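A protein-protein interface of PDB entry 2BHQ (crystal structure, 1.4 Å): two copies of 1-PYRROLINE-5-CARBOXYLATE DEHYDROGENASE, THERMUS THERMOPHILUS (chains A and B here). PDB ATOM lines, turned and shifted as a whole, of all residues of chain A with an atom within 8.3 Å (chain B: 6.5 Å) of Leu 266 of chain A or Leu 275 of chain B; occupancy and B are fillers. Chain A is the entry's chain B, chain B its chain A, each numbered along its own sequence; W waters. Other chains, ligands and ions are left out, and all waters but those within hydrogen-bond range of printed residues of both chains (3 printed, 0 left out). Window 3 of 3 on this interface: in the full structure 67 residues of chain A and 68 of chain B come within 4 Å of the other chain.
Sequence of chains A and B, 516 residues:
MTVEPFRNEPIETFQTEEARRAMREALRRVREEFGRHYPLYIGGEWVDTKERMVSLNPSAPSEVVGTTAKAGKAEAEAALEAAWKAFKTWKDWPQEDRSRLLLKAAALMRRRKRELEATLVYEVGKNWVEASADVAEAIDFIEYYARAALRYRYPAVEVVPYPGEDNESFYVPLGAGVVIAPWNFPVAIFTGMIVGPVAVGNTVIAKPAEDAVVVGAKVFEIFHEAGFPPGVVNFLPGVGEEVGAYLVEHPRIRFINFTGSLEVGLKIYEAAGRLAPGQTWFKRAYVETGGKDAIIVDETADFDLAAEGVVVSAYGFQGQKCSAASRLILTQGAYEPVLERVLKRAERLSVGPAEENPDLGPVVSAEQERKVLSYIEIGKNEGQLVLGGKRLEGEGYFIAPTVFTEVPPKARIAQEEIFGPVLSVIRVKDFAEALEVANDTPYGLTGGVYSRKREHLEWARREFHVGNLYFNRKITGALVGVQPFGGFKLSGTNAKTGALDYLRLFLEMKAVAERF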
ATOM      1  N   PHE A 258      18.223 -21.913  -1.938  1.00  0.00           N
ATOM      2  CA  PHE A 258      16.873 -22.387  -2.219  1.00  0.00           C
ATOM      3  C   PHE A 258      16.763 -23.426  -3.326  1.00  0.00           C
ATOM      4  O   PHE A 258      17.460 -23.358  -4.335  1.00  0.00           O
ATOM      5  CB  PHE A 258      16.007 -21.180  -2.595  1.00  0.00           C
ATOM      6  CG  PHE A 258      14.670 -21.540  -3.194  1.00  0.00           C
ATOM      7  CD1 PHE A 258      13.600 -21.886  -2.382  1.00  0.00           C
ATOM      8  CD2 PHE A 258      14.486 -21.524  -4.575  1.00  0.00           C
ATOM      9  CE1 PHE A 258      12.361 -22.209  -2.937  1.00  0.00           C
ATOM     10  CE2 PHE A 258      13.253 -21.843  -5.142  1.00  0.00           C
ATOM     11  CZ  PHE A 258      12.188 -22.186  -4.320  1.00  0.00           C
ATOM     12  N   GLY A 260      13.413 -25.313  -5.218  1.00  0.00           N
ATOM     13  CA  GLY A 260      11.963 -25.411  -5.256  1.00  0.00           C
ATOM     14  C   GLY A 260      11.396 -24.945  -6.581  1.00  0.00           C
ATOM     15  O   GLY A 260      12.068 -25.014  -7.609  1.00  0.00           O
ATOM     16  N   SER A 261      10.162 -24.452  -6.557  1.00  0.00           N
ATOM     17  CA  SER A 261       9.502 -24.000  -7.777  1.00  0.00           C
ATOM     18  C   SER A 261      10.104 -22.727  -8.352  1.00  0.00           C
ATOM     19  O   SER A 261      10.688 -21.917  -7.633  1.00  0.00           O
ATOM     20  CB  SER A 261       8.014 -23.763  -7.516  1.00  0.00           C
ATOM     21  OG  SER A 261       7.825 -22.618  -6.704  1.00  0.00           O
ATOM     22  N   LEU A 262       9.943 -22.557  -9.659  1.00  0.00           N
ATOM     23  CA  LEU A 262      10.442 -21.374 -10.345  1.00  0.00           C
ATOM     24  C   LEU A 262       9.720 -20.127  -9.833  1.00  0.00           C
ATOM     25  O   LEU A 262      10.329 -19.071  -9.655  1.00  0.00           O
ATOM     26  CB  LEU A 262      10.227 -21.520 -11.852  1.00  0.00           C
ATOM     27  CG  LEU A 262      10.592 -20.309 -12.708  1.00  0.00           C
ATOM     28  CD1 LEU A 262      12.060 -19.936 -12.481  1.00  0.00           C
ATOM     29  CD2 LEU A 262      10.331 -20.632 -14.172  1.00  0.00           C
ATOM     30  N   GLU A 263       8.418 -20.253  -9.598  1.00  0.00           N
ATOM     31  CA  GLU A 263       7.619 -19.140  -9.099  1.00  0.00           C
ATOM     32  C   GLU A 263       8.245 -18.529  -7.849  1.00  0.00           C
ATOM     33  O   GLU A 263       8.440 -17.317  -7.764  1.00  0.00           O
ATOM     34  CB  GLU A 263       6.201 -19.618  -8.773  1.00  0.00           C
ATOM     35  CG  GLU A 263       5.347 -18.576  -8.070  1.00  0.00           C
ATOM     36  CD  GLU A 263       4.014 -19.131  -7.601  1.00  0.00           C
ATOM     37  OE1 GLU A 263       3.187 -19.509  -8.461  1.00  0.00           O
ATOM     38  OE2 GLU A 263       3.797 -19.194  -6.371  1.00  0.00           O
ATOM     39  N   VAL A 264       8.560 -19.380  -6.879  1.00  0.00           N
ATOM     40  CA  VAL A 264       9.160 -18.928  -5.633  1.00  0.00           C
ATOM     41  C   VAL A 264      10.605 -18.482  -5.854  1.00  0.00           C
ATOM     42  O   VAL A 264      11.037 -17.469  -5.304  1.00  0.00           O
ATOM     43  CB  VAL A 264       9.109 -20.052  -4.572  1.00  0.00           C
ATOM     44  CG1 VAL A 264       9.793 -19.602  -3.287  1.00  0.00           C
ATOM     45  CG2 VAL A 264       7.655 -20.418  -4.291  1.00  0.00           C
ATOM     46  N   GLY A 265      11.339 -19.233  -6.671  1.00  0.00           N
ATOM     47  CA  GLY A 265      12.723 -18.892  -6.949  1.00  0.00           C
ATOM     48  C   GLY A 265      12.891 -17.512  -7.563  1.00  0.00           C
ATOM     49  O   GLY A 265      13.845 -16.793  -7.247  1.00  0.00           O
ATOM     50  N   LEU A 266      11.974 -17.138  -8.451  1.00  0.00           N
ATOM     51  CA  LEU A 266      12.037 -15.826  -9.085  1.00  0.00           C
ATOM     52  C   LEU A 266      11.842 -14.730  -8.043  1.00  0.00           C
ATOM     53  O   LEU A 266      12.532 -13.712  -8.065  1.00  0.00           O
ATOM     54  CB  LEU A 266      10.969 -15.709 -10.179  1.00  0.00           C
ATOM     55  CG  LEU A 266      11.213 -16.528 -11.453  1.00  0.00           C
ATOM     56  CD1 LEU A 266       9.984 -16.470 -12.354  1.00  0.00           C
ATOM     57  CD2 LEU A 266      12.434 -15.986 -12.185  1.00  0.00           C
ATOM     58  N   LYS A 267      10.904 -14.943  -7.125  1.00  0.00           N
ATOM     59  CA  LYS A 267      10.642 -13.963  -6.077  1.00  0.00           C
ATOM     60  C   LYS A 267      11.841 -13.830  -5.142  1.00  0.00           C
ATOM     61  O   LYS A 267      12.189 -12.731  -4.714  1.00  0.00           O
ATOM     62  CB  LYS A 267       9.407 -14.365  -5.268  1.00  0.00           C
ATOM     63  CG  LYS A 267       8.112 -14.295  -6.055  1.00  0.00           C
ATOM     64  CD  LYS A 267       6.931 -14.761  -5.218  1.00  0.00           C
ATOM     65  CE  LYS A 267       5.644 -14.725  -6.029  1.00  0.00           C
ATOM     66  NZ  LYS A 267       4.486 -15.240  -5.242  1.00  0.00           N
ATOM     67  N   ILE A 268      12.463 -14.958  -4.819  1.00  0.00           N
ATOM     68  CA  ILE A 268      13.620 -14.954  -3.935  1.00  0.00           C
ATOM     69  C   ILE A 268      14.790 -14.216  -4.579  1.00  0.00           C
ATOM     70  O   ILE A 268      15.435 -13.386  -3.948  1.00  0.00           O
ATOM     71  CB  ILE A 268      14.049 -16.399  -3.577  1.00  0.00           C
ATOM     72  CG1 ILE A 268      13.034 -17.008  -2.605  1.00  0.00           C
ATOM     73  CG2 ILE A 268      15.447 -16.405  -2.964  1.00  0.00           C
ATOM     74  CD1 ILE A 268      13.309 -18.456  -2.250  1.00  0.00           C
ATOM     75  N   TYR A 269      15.044 -14.499  -5.849  1.00  0.00           N
ATOM     76  CA  TYR A 269      16.152 -13.853  -6.536  1.00  0.00           C
ATOM     77  C   TYR A 269      15.925 -12.350  -6.655  1.00  0.00           C
ATOM     78  O   TYR A 269      16.865 -11.559  -6.551  1.00  0.00           O
ATOM     79  CB  TYR A 269      16.333 -14.470  -7.921  1.00  0.00           C
ATOM     80  CG  TYR A 269      17.725 -14.301  -8.489  1.00  0.00           C
ATOM     81  CD1 TYR A 269      17.962 -13.454  -9.570  1.00  0.00           C
ATOM     82  CD2 TYR A 269      18.799 -15.025  -7.969  1.00  0.00           C
ATOM     83  CE1 TYR A 269      19.231 -13.335 -10.128  1.00  0.00           C
ATOM     84  CE2 TYR A 269      20.072 -14.914  -8.515  1.00  0.00           C
ATOM     85  CZ  TYR A 269      20.280 -14.071  -9.598  1.00  0.00           C
ATOM     86  OH  TYR A 269      21.533 -13.984 -10.163  1.00  0.00           O
ATOM     87  N   GLU A 270      14.675 -11.947  -6.867  1.00  0.00           N
ATOM     88  CA  GLU A 270      14.379 -10.526  -6.992  1.00  0.00           C
ATOM     89  C   GLU A 270      14.585  -9.833  -5.648  1.00  0.00           C
ATOM     90  O   GLU A 270      15.188  -8.763  -5.571  1.00  0.00           O
ATOM     91  CB  GLU A 270      12.937 -10.325  -7.470  1.00  0.00           C
ATOM     92  CG  GLU A 270      12.639  -8.897  -7.887  1.00  0.00           C
ATOM     93  CD  GLU A 270      11.258  -8.736  -8.486  1.00  0.00           C
ATOM     94  OE1 GLU A 270      10.877  -9.561  -9.339  1.00  0.00           O
ATOM     95  OE2 GLU A 270      10.557  -7.774  -8.108  1.00  0.00           O
ATOM     96  N   ALA A 271      14.093 -10.456  -4.582  1.00  0.00           N
ATOM     97  CA  ALA A 271      14.229  -9.891  -3.247  1.00  0.00           C
ATOM     98  C   ALA A 271      15.692  -9.812  -2.814  1.00  0.00           C
ATOM     99  O   ALA A 271      16.102  -8.852  -2.160  1.00  0.00           O
ATOM    100  CB  ALA A 271      13.435 -10.726  -2.246  1.00  0.00           C
ATOM    101  N   ALA A 272      16.476 -10.822  -3.177  1.00  0.00           N
ATOM    102  CA  ALA A 272      17.888 -10.861  -2.811  1.00  0.00           C
ATOM    103  C   ALA A 272      18.660  -9.713  -3.456  1.00  0.00           C
ATOM    104  O   ALA A 272      19.694  -9.282  -2.944  1.00  0.00           O
ATOM    105  CB  ALA A 272      18.496 -12.198  -3.220  1.00  0.00           C
ATOM    106  N   GLY A 273      18.145  -9.220  -4.578  1.00  0.00           N
ATOM    107  CA  GLY A 273      18.797  -8.130  -5.282  1.00  0.00           C
ATOM    108  C   GLY A 273      18.571  -6.764  -4.662  1.00  0.00           C
ATOM    109  O   GLY A 273      19.240  -5.799  -5.031  1.00  0.00           O
ATOM    110  N   ARG A 274      17.636  -6.681  -3.720  1.00  0.00           N
ATOM    111  CA  ARG A 274      17.322  -5.417  -3.062  1.00  0.00           C
ATOM    112  C   ARG A 274      18.095  -5.188  -1.772  1.00  0.00           C
ATOM    113  O   ARG A 274      18.415  -6.129  -1.045  1.00  0.00           O
ATOM    114  CB  ARG A 274      15.822  -5.338  -2.745  1.00  0.00           C
ATOM    115  CG  ARG A 274      14.913  -5.365  -3.961  1.00  0.00           C
ATOM    116  CD  ARG A 274      13.515  -4.868  -3.600  1.00  0.00           C
ATOM    117  NE  ARG A 274      12.860  -5.712  -2.604  1.00  0.00           N
ATOM    118  CZ  ARG A 274      12.249  -6.860  -2.877  1.00  0.00           C
ATOM    119  NH1 ARG A 274      11.686  -7.560  -1.900  1.00  0.00           N
ATOM    120  NH2 ARG A 274      12.188  -7.302  -4.126  1.00  0.00           N
ATOM    121  N   VAL A 287      19.691 -20.513  -6.337  1.00  0.00           N
ATOM    122  CA  VAL A 287      18.400 -21.152  -6.546  1.00  0.00           C
ATOM    123  C   VAL A 287      18.420 -22.258  -7.596  1.00  0.00           C
ATOM    124  O   VAL A 287      19.035 -22.121  -8.652  1.00  0.00           O
ATOM    125  CB  VAL A 287      17.323 -20.105  -6.958  1.00  0.00           C
ATOM    126  CG1 VAL A 287      17.252 -18.993  -5.925  1.00  0.00           C
ATOM    127  CG2 VAL A 287      17.646 -19.521  -8.325  1.00  0.00           C
ATOM    128  N   THR A 289      15.624 -24.245  -9.566  1.00  0.00           N
ATOM    129  CA  THR A 289      14.203 -24.056  -9.829  1.00  0.00           C
ATOM    130  C   THR A 289      13.431 -24.966 -10.783  1.00  0.00           C
ATOM    131  O   THR A 289      12.474 -24.512 -11.423  1.00  0.00           O
ATOM    132  CB  THR A 289      13.989 -22.609 -10.289  1.00  0.00           C
ATOM    133  OG1 THR A 289      15.004 -22.278 -11.247  1.00  0.00           O
ATOM    134  CG2 THR A 289      14.098 -21.646  -9.112  1.00  0.00           C
ATOM    135  N   PRO A 442      11.937 -22.917 -21.363  1.00  0.00           N
ATOM    136  CA  PRO A 442      12.624 -21.921 -20.532  1.00  0.00           C
ATOM    137  C   PRO A 442      13.657 -22.548 -19.595  1.00  0.00           C
ATOM    138  O   PRO A 442      14.414 -21.839 -18.933  1.00  0.00           O
ATOM    139  CB  PRO A 442      11.485 -21.287 -19.730  1.00  0.00           C
ATOM    140  CG  PRO A 442      10.243 -21.598 -20.535  1.00  0.00           C
ATOM    141  CD  PRO A 442      10.507 -22.992 -21.018  1.00  0.00           C
ATOM    142  N   TYR A 443      13.674 -23.874 -19.546  1.00  0.00           N
ATOM    143  CA  TYR A 443      14.553 -24.602 -18.636  1.00  0.00           C
ATOM    144  C   TYR A 443      15.812 -25.205 -19.248  1.00  0.00           C
ATOM    145  O   TYR A 443      16.047 -25.107 -20.451  1.00  0.00           O
ATOM    146  CB  TYR A 443      13.747 -25.710 -17.953  1.00  0.00           C
ATOM    147  CG  TYR A 443      12.602 -25.217 -17.094  1.00  0.00           C
ATOM    148  CD1 TYR A 443      11.280 -25.304 -17.537  1.00  0.00           C
ATOM    149  CD2 TYR A 443      12.836 -24.715 -15.815  1.00  0.00           C
ATOM    150  CE1 TYR A 443      10.221 -24.913 -16.719  1.00  0.00           C
ATOM    151  CE2 TYR A 443      11.783 -24.319 -14.989  1.00  0.00           C
ATOM    152  CZ  TYR A 443      10.481 -24.428 -15.447  1.00  0.00           C
ATOM    153  OH  TYR A 443       9.444 -24.086 -14.613  1.00  0.00           O
ATOM    154  N   LYS A 489      19.664 -21.671 -17.652  1.00  0.00           N
ATOM    155  CA  LYS A 489      18.437 -20.927 -17.881  1.00  0.00           C
ATOM    156  C   LYS A 489      17.535 -20.844 -16.655  1.00  0.00           C
ATOM    157  O   LYS A 489      18.024 -20.624 -15.543  1.00  0.00           O
ATOM    158  CB  LYS A 489      17.717 -21.550 -19.083  1.00  0.00           C
ATOM    159  CG  LYS A 489      18.537 -21.388 -20.373  1.00  0.00           C
ATOM    160  CD  LYS A 489      18.218 -22.420 -21.446  1.00  0.00           C
ATOM    161  CE  LYS A 489      16.782 -22.321 -21.931  1.00  0.00           C
ATOM    162  NZ  LYS A 489      16.497 -23.366 -22.958  1.00  0.00           N
ATOM    163  N   LEU A 490      16.229 -21.025 -16.827  1.00  0.00           N
ATOM    164  CA  LEU A 490      15.346 -20.902 -15.676  1.00  0.00           C
ATOM    165  C   LEU A 490      15.315 -22.092 -14.728  1.00  0.00           C
ATOM    166  O   LEU A 490      14.430 -22.196 -13.874  1.00  0.00           O
ATOM    167  CB  LEU A 490      13.935 -20.498 -16.129  1.00  0.00           C
ATOM    168  CG  LEU A 490      13.901 -19.078 -16.728  1.00  0.00           C
ATOM    169  CD1 LEU A 490      12.458 -18.646 -16.976  1.00  0.00           C
ATOM    170  CD2 LEU A 490      14.585 -18.091 -15.788  1.00  0.00           C
ATOM    171  N   ALA B 271      18.157  -4.425 -10.419  1.00  0.00           N
ATOM    172  CA  ALA B 271      17.624  -4.687 -11.752  1.00  0.00           C
ATOM    173  C   ALA B 271      18.006  -6.086 -12.244  1.00  0.00           C
ATOM    174  O   ALA B 271      17.204  -6.771 -12.880  1.00  0.00           O
ATOM    175  CB  ALA B 271      18.134  -3.631 -12.731  1.00  0.00           C
ATOM    176  N   ALA B 272      19.230  -6.511 -11.946  1.00  0.00           N
ATOM    177  CA  ALA B 272      19.705  -7.825 -12.369  1.00  0.00           C
ATOM    178  C   ALA B 272      18.916  -8.956 -11.718  1.00  0.00           C
ATOM    179  O   ALA B 272      18.845 -10.063 -12.254  1.00  0.00           O
ATOM    180  CB  ALA B 272      21.192  -7.977 -12.044  1.00  0.00           C
ATOM    181  N   GLY B 273      18.329  -8.680 -10.558  1.00  0.00           N
ATOM    182  CA  GLY B 273      17.560  -9.697  -9.862  1.00  0.00           C
ATOM    183  C   GLY B 273      16.158  -9.894 -10.408  1.00  0.00           C
ATOM    184  O   GLY B 273      15.460 -10.832 -10.014  1.00  0.00           O
ATOM    185  N   ARG B 274      15.750  -9.022 -11.324  1.00  0.00           N
ATOM    186  CA  ARG B 274      14.418  -9.093 -11.912  1.00  0.00           C
ATOM    187  C   ARG B 274      14.394  -9.850 -13.235  1.00  0.00           C
ATOM    188  O   ARG B 274      15.359  -9.821 -14.005  1.00  0.00           O
ATOM    189  CB  ARG B 274      13.862  -7.680 -12.146  1.00  0.00           C
ATOM    190  CG  ARG B 274      13.742  -6.824 -10.897  1.00  0.00           C
ATOM    191  CD  ARG B 274      12.869  -5.603 -11.159  1.00  0.00           C
ATOM    192  NE  ARG B 274      13.446  -4.693 -12.146  1.00  0.00           N
ATOM    193  CZ  ARG B 274      14.346  -3.751 -11.872  1.00  0.00           C
ATOM    194  NH1 ARG B 274      14.811  -2.977 -12.843  1.00  0.00           N
ATOM    195  NH2 ARG B 274      14.771  -3.572 -10.628  1.00  0.00           N
ATOM    196  N   LEU B 275      13.285 -10.530 -13.496  1.00  0.00           N
ATOM    197  CA  LEU B 275      13.131 -11.260 -14.740  1.00  0.00           C
ATOM    198  C   LEU B 275      12.411 -10.339 -15.721  1.00  0.00           C
ATOM    199  O   LEU B 275      11.209 -10.102 -15.592  1.00  0.00           O
ATOM    200  CB  LEU B 275      12.300 -12.528 -14.526  1.00  0.00           C
ATOM    201  CG  LEU B 275      12.222 -13.471 -15.725  1.00  0.00           C
ATOM    202  CD1 LEU B 275      13.514 -14.277 -15.825  1.00  0.00           C
ATOM    203  CD2 LEU B 275      11.025 -14.400 -15.568  1.00  0.00           C
ATOM    204  N   ALA B 276      13.148  -9.798 -16.684  1.00  0.00           N
ATOM    205  CA  ALA B 276      12.547  -8.920 -17.682  1.00  0.00           C
ATOM    206  C   ALA B 276      11.607  -9.757 -18.541  1.00  0.00           C
ATOM    207  O   ALA B 276      11.774 -10.971 -18.658  1.00  0.00           O
ATOM    208  CB  ALA B 276      13.630  -8.295 -18.545  1.00  0.00           C
ATOM    209  N   PRO B 277      10.596  -9.125 -19.156  1.00  0.00           N
ATOM    210  CA  PRO B 277       9.672  -9.897 -19.992  1.00  0.00           C
ATOM    211  C   PRO B 277      10.387 -10.710 -21.071  1.00  0.00           C
ATOM    212  O   PRO B 277      11.138 -10.160 -21.874  1.00  0.00           O
ATOM    213  CB  PRO B 277       8.771  -8.816 -20.585  1.00  0.00           C
ATOM    214  CG  PRO B 277       8.711  -7.810 -19.479  1.00  0.00           C
ATOM    215  CD  PRO B 277      10.157  -7.723 -19.039  1.00  0.00           C
ATOM    216  N   GLY B 278      10.153 -12.020 -21.078  1.00  0.00           N
ATOM    217  CA  GLY B 278      10.772 -12.885 -22.070  1.00  0.00           C
ATOM    218  C   GLY B 278      12.153 -13.408 -21.711  1.00  0.00           C
ATOM    219  O   GLY B 278      12.720 -14.221 -22.440  1.00  0.00           O
ATOM    220  N   GLN B 279      12.693 -12.944 -20.590  1.00  0.00           N
ATOM    221  CA  GLN B 279      14.020 -13.364 -20.136  1.00  0.00           C
ATOM    222  C   GLN B 279      14.005 -14.853 -19.791  1.00  0.00           C
ATOM    223  O   GLN B 279      13.068 -15.332 -19.155  1.00  0.00           O
ATOM    224  CB  GLN B 279      14.412 -12.534 -18.913  1.00  0.00           C
ATOM    225  CG  GLN B 279      15.848 -12.686 -18.449  1.00  0.00           C
ATOM    226  CD  GLN B 279      16.179 -11.696 -17.348  1.00  0.00           C
ATOM    227  OE1 GLN B 279      15.966 -10.492 -17.504  1.00  0.00           O
ATOM    228  NE2 GLN B 279      16.697 -12.195 -16.227  1.00  0.00           N
ATOM    229  N   THR B 280      15.045 -15.580 -20.199  1.00  0.00           N
ATOM    230  CA  THR B 280      15.105 -17.021 -19.944  1.00  0.00           C
ATOM    231  C   THR B 280      16.286 -17.494 -19.096  1.00  0.00           C
ATOM    232  O   THR B 280      16.776 -18.614 -19.260  1.00  0.00           O
ATOM    233  CB  THR B 280      15.104 -17.812 -21.270  1.00  0.00           C
ATOM    234  OG1 THR B 280      16.191 -17.374 -22.093  1.00  0.00           O
ATOM    235  CG2 THR B 280      13.791 -17.601 -22.014  1.00  0.00           C
ATOM    236  N   TRP B 281      16.740 -16.643 -18.185  1.00  0.00           N
ATOM    237  CA  TRP B 281      17.842 -17.001 -17.299  1.00  0.00           C
ATOM    238  C   TRP B 281      17.914 -16.055 -16.117  1.00  0.00           C
ATOM    239  O   TRP B 281      17.251 -15.012 -16.101  1.00  0.00           O
ATOM    240  CB  TRP B 281      19.185 -16.973 -18.053  1.00  0.00           C
ATOM    241  CG  TRP B 281      19.493 -15.668 -18.749  1.00  0.00           C
ATOM    242  CD1 TRP B 281      19.656 -14.437 -18.171  1.00  0.00           C
ATOM    243  CD2 TRP B 281      19.677 -15.477 -20.155  1.00  0.00           C
ATOM    244  NE1 TRP B 281      19.930 -13.491 -19.136  1.00  0.00           N
ATOM    245  CE2 TRP B 281      19.950 -14.104 -20.362  1.00  0.00           C
ATOM    246  CE3 TRP B 281      19.642 -16.334 -21.260  1.00  0.00           C
ATOM    247  CZ2 TRP B 281      20.186 -13.569 -21.634  1.00  0.00           C
ATOM    248  CZ3 TRP B 281      19.877 -15.800 -22.531  1.00  0.00           C
ATOM    249  CH2 TRP B 281      20.145 -14.429 -22.703  1.00  0.00           C
ATOM    250  N   PHE B 282      18.702 -16.434 -15.116  1.00  0.00           N
ATOM    251  CA  PHE B 282      18.914 -15.596 -13.945  1.00  0.00           C
ATOM    252  C   PHE B 282      20.201 -14.834 -14.256  1.00  0.00           C
ATOM    253  O   PHE B 282      21.271 -15.428 -14.398  1.00  0.00           O
ATOM    254  CB  PHE B 282      19.093 -16.444 -12.679  1.00  0.00           C
ATOM    255  CG  PHE B 282      17.826 -17.104 -12.202  1.00  0.00           C
ATOM    256  CD1 PHE B 282      17.403 -18.312 -12.747  1.00  0.00           C
ATOM    257  CD2 PHE B 282      17.043 -16.500 -11.221  1.00  0.00           C
ATOM    258  CE1 PHE B 282      16.220 -18.910 -12.323  1.00  0.00           C
ATOM    259  CE2 PHE B 282      15.859 -17.086 -10.791  1.00  0.00           C
ATOM    260  CZ  PHE B 282      15.444 -18.295 -11.342  1.00  0.00           C
HETATM  261  O   HOH W   1      20.088 -18.888 -15.418  1.00  0.00           O
HETATM  262  O   HOH W   2      11.521 -11.285 -11.343  1.00  0.00           O
HETATM  263  O   HOH W   3      13.763 -12.859 -10.445  1.00  0.00           O
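Among the printed residues, merely in contact across the chains: Leu 262 of chain A with Phe 282 of chain B, Leu 266 of chain A with Leu 275 of chain B, Leu 266 of chain A with Phe 282 of chain B, Tyr 269 of chain A with Ala 272 of chain B, Tyr 269 of chain A with Gly 273 of chain B, Tyr 269 of chain A with Phe 282 of chain B, Glu 270 of chain A with Arg 274 of chain B, Val 287 of chain A with Phe 282 of chain B, Thr 289 of chain A with Phe 282 of chain B, Lys 489 of chain A with Thr 280 of chain B, Lys 489 of chain A with Trp 281 of chain B, Lys 489 of chain A with Phe 282 of chain B, Leu 490 of chain A with Leu 275 of chain B, Leu 490 of chain A with Trp 281 of chain B and Leu 490 of chain A with Phe 282 of chain B.
Water W3 lies within hydrogen-bond range of the backbone carbonyl oxygen of Gly 273 of chain B (2.7 Å) and the backbone carbonyl oxygen of Leu 266 of chain A (2.8 Å).
Water W1 bridges O of Lys 489 of chain A and N of Phe 282 of chain B.
Water W2 lies within hydrogen-bond range of OE1 of Glu 270 of chain A and N of Leu 275 of chain B.
4 positions are printed for both chains.
Of the 17 pairs that touch across the chains among the printed residues, none has its exchanged pair printed and touching as well.
Of the 12 printed residues of chain B, 7 touch a printed residue of chain A.
Among the printed residues, 17 pairs touch across the chains.
Among the printed residues, no Asp or Glu carboxylate lies within 4 Å of a Lys or Arg side-chain nitrogen of the other chain.
The side-chain hydroxyl (OG1) of Thr 289 of chain A is in hydrogen-bond range of the backbone carbonyl oxygen (O) of Leu 490 of chain A, 2.7 Å away.
The backbone carbonyl oxygen (O) of Pro 442 of chain A sits at hydrogen-bond distance from the backbone NH (N) of Leu 490 of chain A (2.9 Å).
O of Trp 281 of chain B sits at hydrogen-bond distance from NE2 of Gln 279 of chain B.
NZ of Lys 489 of chain A is in hydrogen-bond range of O of Tyr 443 of chain A.
The backbone NH (N) of Glu 270 of chain A sits close to the backbone carbonyl oxygen (O) of Gly 273 of chain B, at 3.4 Å.
O of Thr 280 of chain B lies within hydrogen-bond range of N of Leu 490 of chain A.
Gly 260 of chain A touches none of the printed residues of chain B.
Printed residues of chain B within 4 Å of Leu 262 of chain A: Phe 282.
Gly 265 of chain A touches none of the printed residues of chain B.
Of chain B, only Leu 275 (3.96 Å) and Phe 282 (3.9 Å) come within 4 Å of Leu 266 of chain A.
Of the printed residues of chain B, Tyr 269 of chain A touches Ala 272 (3.9 Å), Gly 273 (3.7 Å) and Phe 282 (3.6 Å).
Of chain A, only Leu 266 (3.96 Å) and Leu 490 (3.96 Å) come within 4 Å of Leu 275 of chain B.
The nearest residue of chain A that does not touch Leu 275 of chain B is Glu 270 of chain A (4.9 Å).
The nearest printed residue of chain A that does not touch Arg 274 of chain B is Tyr 269 of chain A (5.3 Å).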
